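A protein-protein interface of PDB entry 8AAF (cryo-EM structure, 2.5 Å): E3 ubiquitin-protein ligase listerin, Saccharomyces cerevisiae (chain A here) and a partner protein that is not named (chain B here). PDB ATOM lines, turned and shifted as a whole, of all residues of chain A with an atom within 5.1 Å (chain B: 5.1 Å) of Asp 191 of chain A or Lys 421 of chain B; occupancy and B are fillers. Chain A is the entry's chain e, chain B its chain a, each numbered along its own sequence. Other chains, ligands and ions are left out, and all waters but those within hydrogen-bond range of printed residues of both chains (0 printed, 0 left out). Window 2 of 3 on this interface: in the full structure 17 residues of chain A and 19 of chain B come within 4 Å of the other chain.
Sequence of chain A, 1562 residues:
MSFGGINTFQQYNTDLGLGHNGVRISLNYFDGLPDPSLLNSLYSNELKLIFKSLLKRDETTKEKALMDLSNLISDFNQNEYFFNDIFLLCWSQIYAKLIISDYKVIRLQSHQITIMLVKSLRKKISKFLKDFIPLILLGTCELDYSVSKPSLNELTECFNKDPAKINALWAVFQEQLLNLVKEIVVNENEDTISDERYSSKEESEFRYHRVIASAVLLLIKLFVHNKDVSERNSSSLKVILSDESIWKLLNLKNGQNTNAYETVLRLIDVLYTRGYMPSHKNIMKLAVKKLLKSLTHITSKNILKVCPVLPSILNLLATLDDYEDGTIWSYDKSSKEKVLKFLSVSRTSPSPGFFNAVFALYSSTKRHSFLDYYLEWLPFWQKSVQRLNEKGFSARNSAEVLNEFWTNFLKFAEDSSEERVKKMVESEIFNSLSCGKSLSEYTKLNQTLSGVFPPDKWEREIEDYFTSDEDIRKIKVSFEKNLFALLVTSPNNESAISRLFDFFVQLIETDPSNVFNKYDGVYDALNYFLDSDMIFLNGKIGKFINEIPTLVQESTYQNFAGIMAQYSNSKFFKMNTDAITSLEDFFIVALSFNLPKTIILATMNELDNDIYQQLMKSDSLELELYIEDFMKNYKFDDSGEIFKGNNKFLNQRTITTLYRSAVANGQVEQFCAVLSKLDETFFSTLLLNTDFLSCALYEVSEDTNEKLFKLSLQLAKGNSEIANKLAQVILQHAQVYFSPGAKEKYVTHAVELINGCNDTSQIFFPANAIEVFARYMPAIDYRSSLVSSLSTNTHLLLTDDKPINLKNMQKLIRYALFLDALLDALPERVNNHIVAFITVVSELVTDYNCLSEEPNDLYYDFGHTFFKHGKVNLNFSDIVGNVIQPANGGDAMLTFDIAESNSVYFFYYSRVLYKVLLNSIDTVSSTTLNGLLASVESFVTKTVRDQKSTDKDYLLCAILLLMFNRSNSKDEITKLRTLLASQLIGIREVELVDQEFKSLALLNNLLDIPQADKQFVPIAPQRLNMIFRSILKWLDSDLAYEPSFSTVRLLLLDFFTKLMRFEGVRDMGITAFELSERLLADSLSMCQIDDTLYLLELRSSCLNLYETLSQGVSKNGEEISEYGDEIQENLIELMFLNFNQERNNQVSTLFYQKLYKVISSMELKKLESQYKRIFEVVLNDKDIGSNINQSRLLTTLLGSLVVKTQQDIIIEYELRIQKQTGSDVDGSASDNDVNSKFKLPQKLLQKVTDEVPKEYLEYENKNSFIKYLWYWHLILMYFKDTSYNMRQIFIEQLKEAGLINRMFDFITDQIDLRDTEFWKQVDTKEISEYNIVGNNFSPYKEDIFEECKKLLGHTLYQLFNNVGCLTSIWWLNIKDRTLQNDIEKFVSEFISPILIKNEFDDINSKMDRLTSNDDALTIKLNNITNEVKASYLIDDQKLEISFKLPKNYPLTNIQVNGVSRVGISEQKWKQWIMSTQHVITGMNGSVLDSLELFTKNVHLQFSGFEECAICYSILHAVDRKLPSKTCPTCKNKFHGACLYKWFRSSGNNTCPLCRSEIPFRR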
ATOM      1  N   TYR A  29     -24.618  -3.771   5.169  1.00  0.00           N
ATOM      2  CA  TYR A  29     -24.868  -3.283   3.821  1.00  0.00           C
ATOM      3  C   TYR A  29     -25.675  -4.214   2.946  1.00  0.00           C
ATOM      4  O   TYR A  29     -26.522  -3.763   2.191  1.00  0.00           O
ATOM      5  CB  TYR A  29     -23.552  -2.899   3.136  1.00  0.00           C
ATOM      6  CG  TYR A  29     -22.589  -4.022   2.834  1.00  0.00           C
ATOM      7  CD1 TYR A  29     -21.723  -4.497   3.801  1.00  0.00           C
ATOM      8  CD2 TYR A  29     -22.517  -4.575   1.567  1.00  0.00           C
ATOM      9  CE1 TYR A  29     -20.836  -5.515   3.526  1.00  0.00           C
ATOM     10  CE2 TYR A  29     -21.634  -5.592   1.283  1.00  0.00           C
ATOM     11  CZ  TYR A  29     -20.796  -6.056   2.266  1.00  0.00           C
ATOM     12  OH  TYR A  29     -19.911  -7.064   1.981  1.00  0.00           O
ATOM     13  N   PHE A  30     -25.422  -5.508   3.032  1.00  0.00           N
ATOM     14  CA  PHE A  30     -26.099  -6.450   2.150  1.00  0.00           C
ATOM     15  C   PHE A  30     -27.611  -6.563   2.289  1.00  0.00           C
ATOM     16  O   PHE A  30     -28.302  -6.722   1.292  1.00  0.00           O
ATOM     17  CB  PHE A  30     -25.431  -7.833   2.153  1.00  0.00           C
ATOM     18  CG  PHE A  30     -24.940  -8.286   3.489  1.00  0.00           C
ATOM     19  CD1 PHE A  30     -23.659  -7.982   3.907  1.00  0.00           C
ATOM     20  CD2 PHE A  30     -25.740  -9.053   4.304  1.00  0.00           C
ATOM     21  CE1 PHE A  30     -23.199  -8.410   5.131  1.00  0.00           C
ATOM     22  CE2 PHE A  30     -25.288  -9.485   5.529  1.00  0.00           C
ATOM     23  CZ  PHE A  30     -24.015  -9.164   5.944  1.00  0.00           C
ATOM     24  N   ASN A 189     -20.458  -8.063  12.571  1.00  0.00           N
ATOM     25  CA  ASN A 189     -19.027  -8.335  12.614  1.00  0.00           C
ATOM     26  C   ASN A 189     -18.459  -7.218  11.783  1.00  0.00           C
ATOM     27  O   ASN A 189     -19.205  -6.507  11.137  1.00  0.00           O
ATOM     28  CB  ASN A 189     -18.693  -9.663  11.961  1.00  0.00           C
ATOM     29  CG  ASN A 189     -19.243 -10.847  12.728  1.00  0.00           C
ATOM     30  OD1 ASN A 189     -19.694 -11.826  12.135  1.00  0.00           O
ATOM     31  ND2 ASN A 189     -19.214 -10.762  14.052  1.00  0.00           N
ATOM     32  N   GLU A 190     -17.156  -7.023  11.795  1.00  0.00           N
ATOM     33  CA  GLU A 190     -16.583  -5.900  11.074  1.00  0.00           C
ATOM     34  C   GLU A 190     -16.881  -6.000   9.597  1.00  0.00           C
ATOM     35  O   GLU A 190     -17.192  -5.002   8.953  1.00  0.00           O
ATOM     36  CB  GLU A 190     -15.074  -5.869  11.259  1.00  0.00           C
ATOM     37  CG  GLU A 190     -14.623  -5.756  12.705  1.00  0.00           C
ATOM     38  CD  GLU A 190     -14.341  -7.103  13.335  1.00  0.00           C
ATOM     39  OE1 GLU A 190     -14.250  -8.102  12.590  1.00  0.00           O
ATOM     40  OE2 GLU A 190     -14.209  -7.164  14.575  1.00  0.00           O
ATOM     41  N   ASP A 191     -16.790  -7.203   9.054  1.00  0.00           N
ATOM     42  CA  ASP A 191     -17.060  -7.411   7.640  1.00  0.00           C
ATOM     43  C   ASP A 191     -18.488  -7.085   7.262  1.00  0.00           C
ATOM     44  O   ASP A 191     -18.740  -6.517   6.211  1.00  0.00           O
ATOM     45  CB  ASP A 191     -16.781  -8.855   7.270  1.00  0.00           C
ATOM     46  CG  ASP A 191     -15.338  -9.243   7.502  1.00  0.00           C
ATOM     47  OD1 ASP A 191     -14.511  -8.343   7.755  1.00  0.00           O
ATOM     48  OD2 ASP A 191     -15.029 -10.451   7.430  1.00  0.00           O
ATOM     49  N   THR A 192     -19.433  -7.465   8.104  1.00  0.00           N
ATOM     50  CA  THR A 192     -20.816  -7.215   7.792  1.00  0.00           C
ATOM     51  C   THR A 192     -21.095  -5.724   7.724  1.00  0.00           C
ATOM     52  O   THR A 192     -21.829  -5.275   6.861  1.00  0.00           O
ATOM     53  CB  THR A 192     -21.743  -7.884   8.801  1.00  0.00           C
ATOM     54  OG1 THR A 192     -21.598  -7.249  10.072  1.00  0.00           O
ATOM     55  CG2 THR A 192     -21.405  -9.353   8.933  1.00  0.00           C
ATOM     56  N   ILE A 193     -20.533  -4.953   8.638  1.00  0.00           N
ATOM     57  CA  ILE A 193     -20.751  -3.512   8.645  1.00  0.00           C
ATOM     58  C   ILE A 193     -20.186  -2.797   7.431  1.00  0.00           C
ATOM     59  O   ILE A 193     -20.844  -1.940   6.854  1.00  0.00           O
ATOM     60  CB  ILE A 193     -20.175  -2.873   9.923  1.00  0.00           C
ATOM     61  CG1 ILE A 193     -20.865  -3.439  11.159  1.00  0.00           C
ATOM     62  CG2 ILE A 193     -20.322  -1.362   9.908  1.00  0.00           C
ATOM     63  CD1 ILE A 193     -22.288  -2.959  11.326  1.00  0.00           C
ATOM     64  N   SER A 194     -18.982  -3.160   7.013  1.00  0.00           N
ATOM     65  CA  SER A 194     -18.339  -2.445   5.915  1.00  0.00           C
ATOM     66  C   SER A 194     -17.875  -3.359   4.805  1.00  0.00           C
ATOM     67  O   SER A 194     -17.284  -4.396   5.063  1.00  0.00           O
ATOM     68  CB  SER A 194     -17.124  -1.689   6.438  1.00  0.00           C
ATOM     69  OG  SER A 194     -17.376  -1.122   7.709  1.00  0.00           O
ATOM     70  N   ASP A 195     -18.101  -2.961   3.562  1.00  0.00           N
ATOM     71  CA  ASP A 195     -17.730  -3.811   2.442  1.00  0.00           C
ATOM     72  C   ASP A 195     -16.238  -4.016   2.348  1.00  0.00           C
ATOM     73  O   ASP A 195     -15.470  -3.063   2.385  1.00  0.00           O
ATOM     74  CB  ASP A 195     -18.235  -3.208   1.142  1.00  0.00           C
ATOM     75  CG  ASP A 195     -18.275  -4.207   0.008  1.00  0.00           C
ATOM     76  OD1 ASP A 195     -18.018  -5.406   0.238  1.00  0.00           O
ATOM     77  OD2 ASP A 195     -18.580  -3.787  -1.123  1.00  0.00           O
ATOM     78  N   GLU A 196     -15.825  -5.263   2.184  1.00  0.00           N
ATOM     79  CA  GLU A 196     -14.410  -5.585   2.078  1.00  0.00           C
ATOM     80  C   GLU A 196     -13.731  -5.016   0.857  1.00  0.00           C
ATOM     81  O   GLU A 196     -12.586  -4.607   0.919  1.00  0.00           O
ATOM     82  CB  GLU A 196     -14.235  -7.096   2.102  1.00  0.00           C
ATOM     83  CG  GLU A 196     -15.334  -7.845   1.367  1.00  0.00           C
ATOM     84  CD  GLU A 196     -15.304  -9.332   1.644  1.00  0.00           C
ATOM     85  OE1 GLU A 196     -14.409  -9.778   2.389  1.00  0.00           O
ATOM     86  OE2 GLU A 196     -16.177 -10.053   1.118  1.00  0.00           O
ATOM     87  N   ASN B 417     -21.155  -9.465  -5.608  1.00  0.00           N
ATOM     88  CA  ASN B 417     -20.456  -9.801  -4.375  1.00  0.00           C
ATOM     89  C   ASN B 417     -21.345  -9.559  -3.163  1.00  0.00           C
ATOM     90  O   ASN B 417     -21.293 -10.316  -2.188  1.00  0.00           O
ATOM     91  CB  ASN B 417     -19.165  -8.998  -4.277  1.00  0.00           C
ATOM     92  CG  ASN B 417     -18.141  -9.434  -5.298  1.00  0.00           C
ATOM     93  OD1 ASN B 417     -17.589  -8.615  -6.030  1.00  0.00           O
ATOM     94  ND2 ASN B 417     -17.902 -10.737  -5.373  1.00  0.00           N
ATOM     95  N   THR B 418     -22.186  -8.523  -3.219  1.00  0.00           N
ATOM     96  CA  THR B 418     -23.177  -8.321  -2.171  1.00  0.00           C
ATOM     97  C   THR B 418     -24.225  -9.425  -2.162  1.00  0.00           C
ATOM     98  O   THR B 418     -24.702  -9.800  -1.086  1.00  0.00           O
ATOM     99  CB  THR B 418     -23.863  -6.970  -2.340  1.00  0.00           C
ATOM    100  OG1 THR B 418     -24.543  -6.942  -3.597  1.00  0.00           O
ATOM    101  CG2 THR B 418     -22.843  -5.857  -2.321  1.00  0.00           C
ATOM    102  N   ILE B 419     -24.564  -9.973  -3.330  1.00  0.00           N
ATOM    103  CA  ILE B 419     -25.459 -11.126  -3.380  1.00  0.00           C
ATOM    104  C   ILE B 419     -24.804 -12.346  -2.740  1.00  0.00           C
ATOM    105  O   ILE B 419     -25.451 -13.061  -1.965  1.00  0.00           O
ATOM    106  CB  ILE B 419     -25.895 -11.402  -4.832  1.00  0.00           C
ATOM    107  CG1 ILE B 419     -26.845 -10.306  -5.316  1.00  0.00           C
ATOM    108  CG2 ILE B 419     -26.571 -12.756  -4.973  1.00  0.00           C
ATOM    109  CD1 ILE B 419     -27.317 -10.487  -6.745  1.00  0.00           C
ATOM    110  N   GLU B 420     -23.514 -12.570  -3.004  1.00  0.00           N
ATOM    111  CA  GLU B 420     -22.809 -13.688  -2.371  1.00  0.00           C
ATOM    112  C   GLU B 420     -22.693 -13.505  -0.860  1.00  0.00           C
ATOM    113  O   GLU B 420     -22.797 -14.479  -0.103  1.00  0.00           O
ATOM    114  CB  GLU B 420     -21.430 -13.869  -3.001  1.00  0.00           C
ATOM    115  CG  GLU B 420     -21.467 -14.436  -4.410  1.00  0.00           C
ATOM    116  CD  GLU B 420     -20.202 -14.153  -5.193  1.00  0.00           C
ATOM    117  OE1 GLU B 420     -19.106 -14.233  -4.602  1.00  0.00           O
ATOM    118  OE2 GLU B 420     -20.302 -13.865  -6.404  1.00  0.00           O
ATOM    119  N   LYS B 421     -22.498 -12.265  -0.400  1.00  0.00           N
ATOM    120  CA  LYS B 421     -22.456 -12.010   1.038  1.00  0.00           C
ATOM    121  C   LYS B 421     -23.824 -12.218   1.676  1.00  0.00           C
ATOM    122  O   LYS B 421     -23.924 -12.708   2.810  1.00  0.00           O
ATOM    123  CB  LYS B 421     -21.943 -10.595   1.305  1.00  0.00           C
ATOM    124  CG  LYS B 421     -20.477 -10.404   0.953  1.00  0.00           C
ATOM    125  CD  LYS B 421     -19.560 -11.185   1.876  1.00  0.00           C
ATOM    126  CE  LYS B 421     -19.757 -10.781   3.323  1.00  0.00           C
ATOM    127  NZ  LYS B 421     -19.367  -9.360   3.519  1.00  0.00           N
ATOM    128  N   LEU B 422     -24.890 -11.872   0.950  1.00  0.00           N
ATOM    129  CA  LEU B 422     -26.242 -12.179   1.397  1.00  0.00           C
ATOM    130  C   LEU B 422     -26.503 -13.678   1.459  1.00  0.00           C
ATOM    131  O   LEU B 422     -27.239 -14.129   2.343  1.00  0.00           O
ATOM    132  CB  LEU B 422     -27.253 -11.504   0.471  1.00  0.00           C
ATOM    133  CG  LEU B 422     -28.731 -11.633   0.834  1.00  0.00           C
ATOM    134  CD1 LEU B 422     -28.981 -11.082   2.216  1.00  0.00           C
ATOM    135  CD2 LEU B 422     -29.589 -10.920  -0.178  1.00  0.00           C
ATOM    136  N   ILE B 423     -25.915 -14.454   0.551  1.00  0.00           N
ATOM    137  CA  ILE B 423     -26.057 -15.906   0.619  1.00  0.00           C
ATOM    138  C   ILE B 423     -25.315 -16.463   1.830  1.00  0.00           C
ATOM    139  O   ILE B 423     -25.841 -17.326   2.544  1.00  0.00           O
ATOM    140  CB  ILE B 423     -25.589 -16.562  -0.695  1.00  0.00           C
ATOM    141  CG1 ILE B 423     -26.475 -16.118  -1.854  1.00  0.00           C
ATOM    142  CG2 ILE B 423     -25.648 -18.079  -0.604  1.00  0.00           C
ATOM    143  CD1 ILE B 423     -27.926 -16.483  -1.684  1.00  0.00           C
ATOM    144  N   LYS B 424     -24.104 -15.953   2.097  1.00  0.00           N
ATOM    145  CA  LYS B 424     -23.334 -16.403   3.260  1.00  0.00           C
ATOM    146  C   LYS B 424     -24.040 -16.086   4.572  1.00  0.00           C
ATOM    147  O   LYS B 424     -24.084 -16.927   5.482  1.00  0.00           O
ATOM    148  CB  LYS B 424     -21.942 -15.771   3.273  1.00  0.00           C
ATOM    149  CG  LYS B 424     -21.062 -16.151   2.119  1.00  0.00           C
ATOM    150  CD  LYS B 424     -19.656 -15.616   2.276  1.00  0.00           C
ATOM    151  CE  LYS B 424     -18.872 -15.783   0.986  1.00  0.00           C
ATOM    152  NZ  LYS B 424     -17.483 -15.265   1.106  1.00  0.00           N
ATOM    153  N   SER B 425     -24.606 -14.880   4.684  1.00  0.00           N
ATOM    154  CA  SER B 425     -25.279 -14.495   5.920  1.00  0.00           C
ATOM    155  C   SER B 425     -26.541 -15.316   6.153  1.00  0.00           C
ATOM    156  O   SER B 425     -26.825 -15.717   7.286  1.00  0.00           O
ATOM    157  CB  SER B 425     -25.609 -13.009   5.894  1.00  0.00           C
ATOM    158  OG  SER B 425     -26.568 -12.682   6.881  1.00  0.00           O
ATOM    159  N   GLU B 426     -27.299 -15.600   5.095  1.00  0.00           N
ATOM    160  CA  GLU B 426     -28.500 -16.407   5.270  1.00  0.00           C
ATOM    161  C   GLU B 426     -28.171 -17.877   5.508  1.00  0.00           C
ATOM    162  O   GLU B 426     -28.946 -18.581   6.166  1.00  0.00           O
ATOM    163  CB  GLU B 426     -29.428 -16.239   4.069  1.00  0.00           C
ATOM    164  CG  GLU B 426     -30.050 -14.858   3.958  1.00  0.00           C
ATOM    165  CD  GLU B 426     -30.967 -14.530   5.123  1.00  0.00           C
ATOM    166  OE1 GLU B 426     -31.629 -15.453   5.644  1.00  0.00           O
ATOM    167  OE2 GLU B 426     -31.023 -13.349   5.524  1.00  0.00           O
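OH of Tyr 29 of chain A is in hydrogen-bond range of OD1 of Asp 195 of chain A (3.1 Å).
Of the 10 printed residues of chain A, 4 touch a printed residue of chain B.
Along chain A the printed residues that touch a printed residue of chain B span positions 29 to 196.
Tyr 29 of chain A touches Thr 418 of chain B.
CB of Phe 30 of chain A touches O of Thr 418 of chain B (3.9 Å).
Phe 30 of chain A touches Ser 425 of chain B.
Lys 421 of chain B touches Asp 191 of chain A (NZ to O, 3.97 Å).
Glu 196 of chain A touches Lys 421 of chain B (OE2 to CD, 3.6 Å).
The side-chain amino group (NZ) of Lys 421 of chain B sits at hydrogen-bond distance from the side-chain hydroxyl (OH) of Tyr 29 of chain A (2.8 Å).
Printed residues of chain B within 4 Å of Tyr 29 of chain A: Thr 418 and Lys 421.
Printed residues of chain B within 4 Å of Phe 30 of chain A: Thr 418 (3.9 Å) and Ser 425 (3.6 Å).
Of chain B, only Lys 421 comes within 4 Å of Asp 191 of chain A.
Ser 194 of chain A touches none of the printed residues of chain B.
Of the printed residues of chain B, Glu 196 of chain A touches Lys 421.
Of the printed residues of chain A, Thr 418 of chain B touches Tyr 29 (3.8 Å) and Phe 30 (3.9 Å).
Lys 421 of chain B touches just these residues of chain A: Tyr 29 (2.8 Å), Asp 191 (3.97 Å) and Glu 196 (3.6 Å).
Of the printed residues of chain A, Ser 425 of chain B touches Phe 30 (3.6 Å).
The nearest printed residue of chain B that does not touch Asp 191 of chain A is Lys 424 of chain B (8.3 Å).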
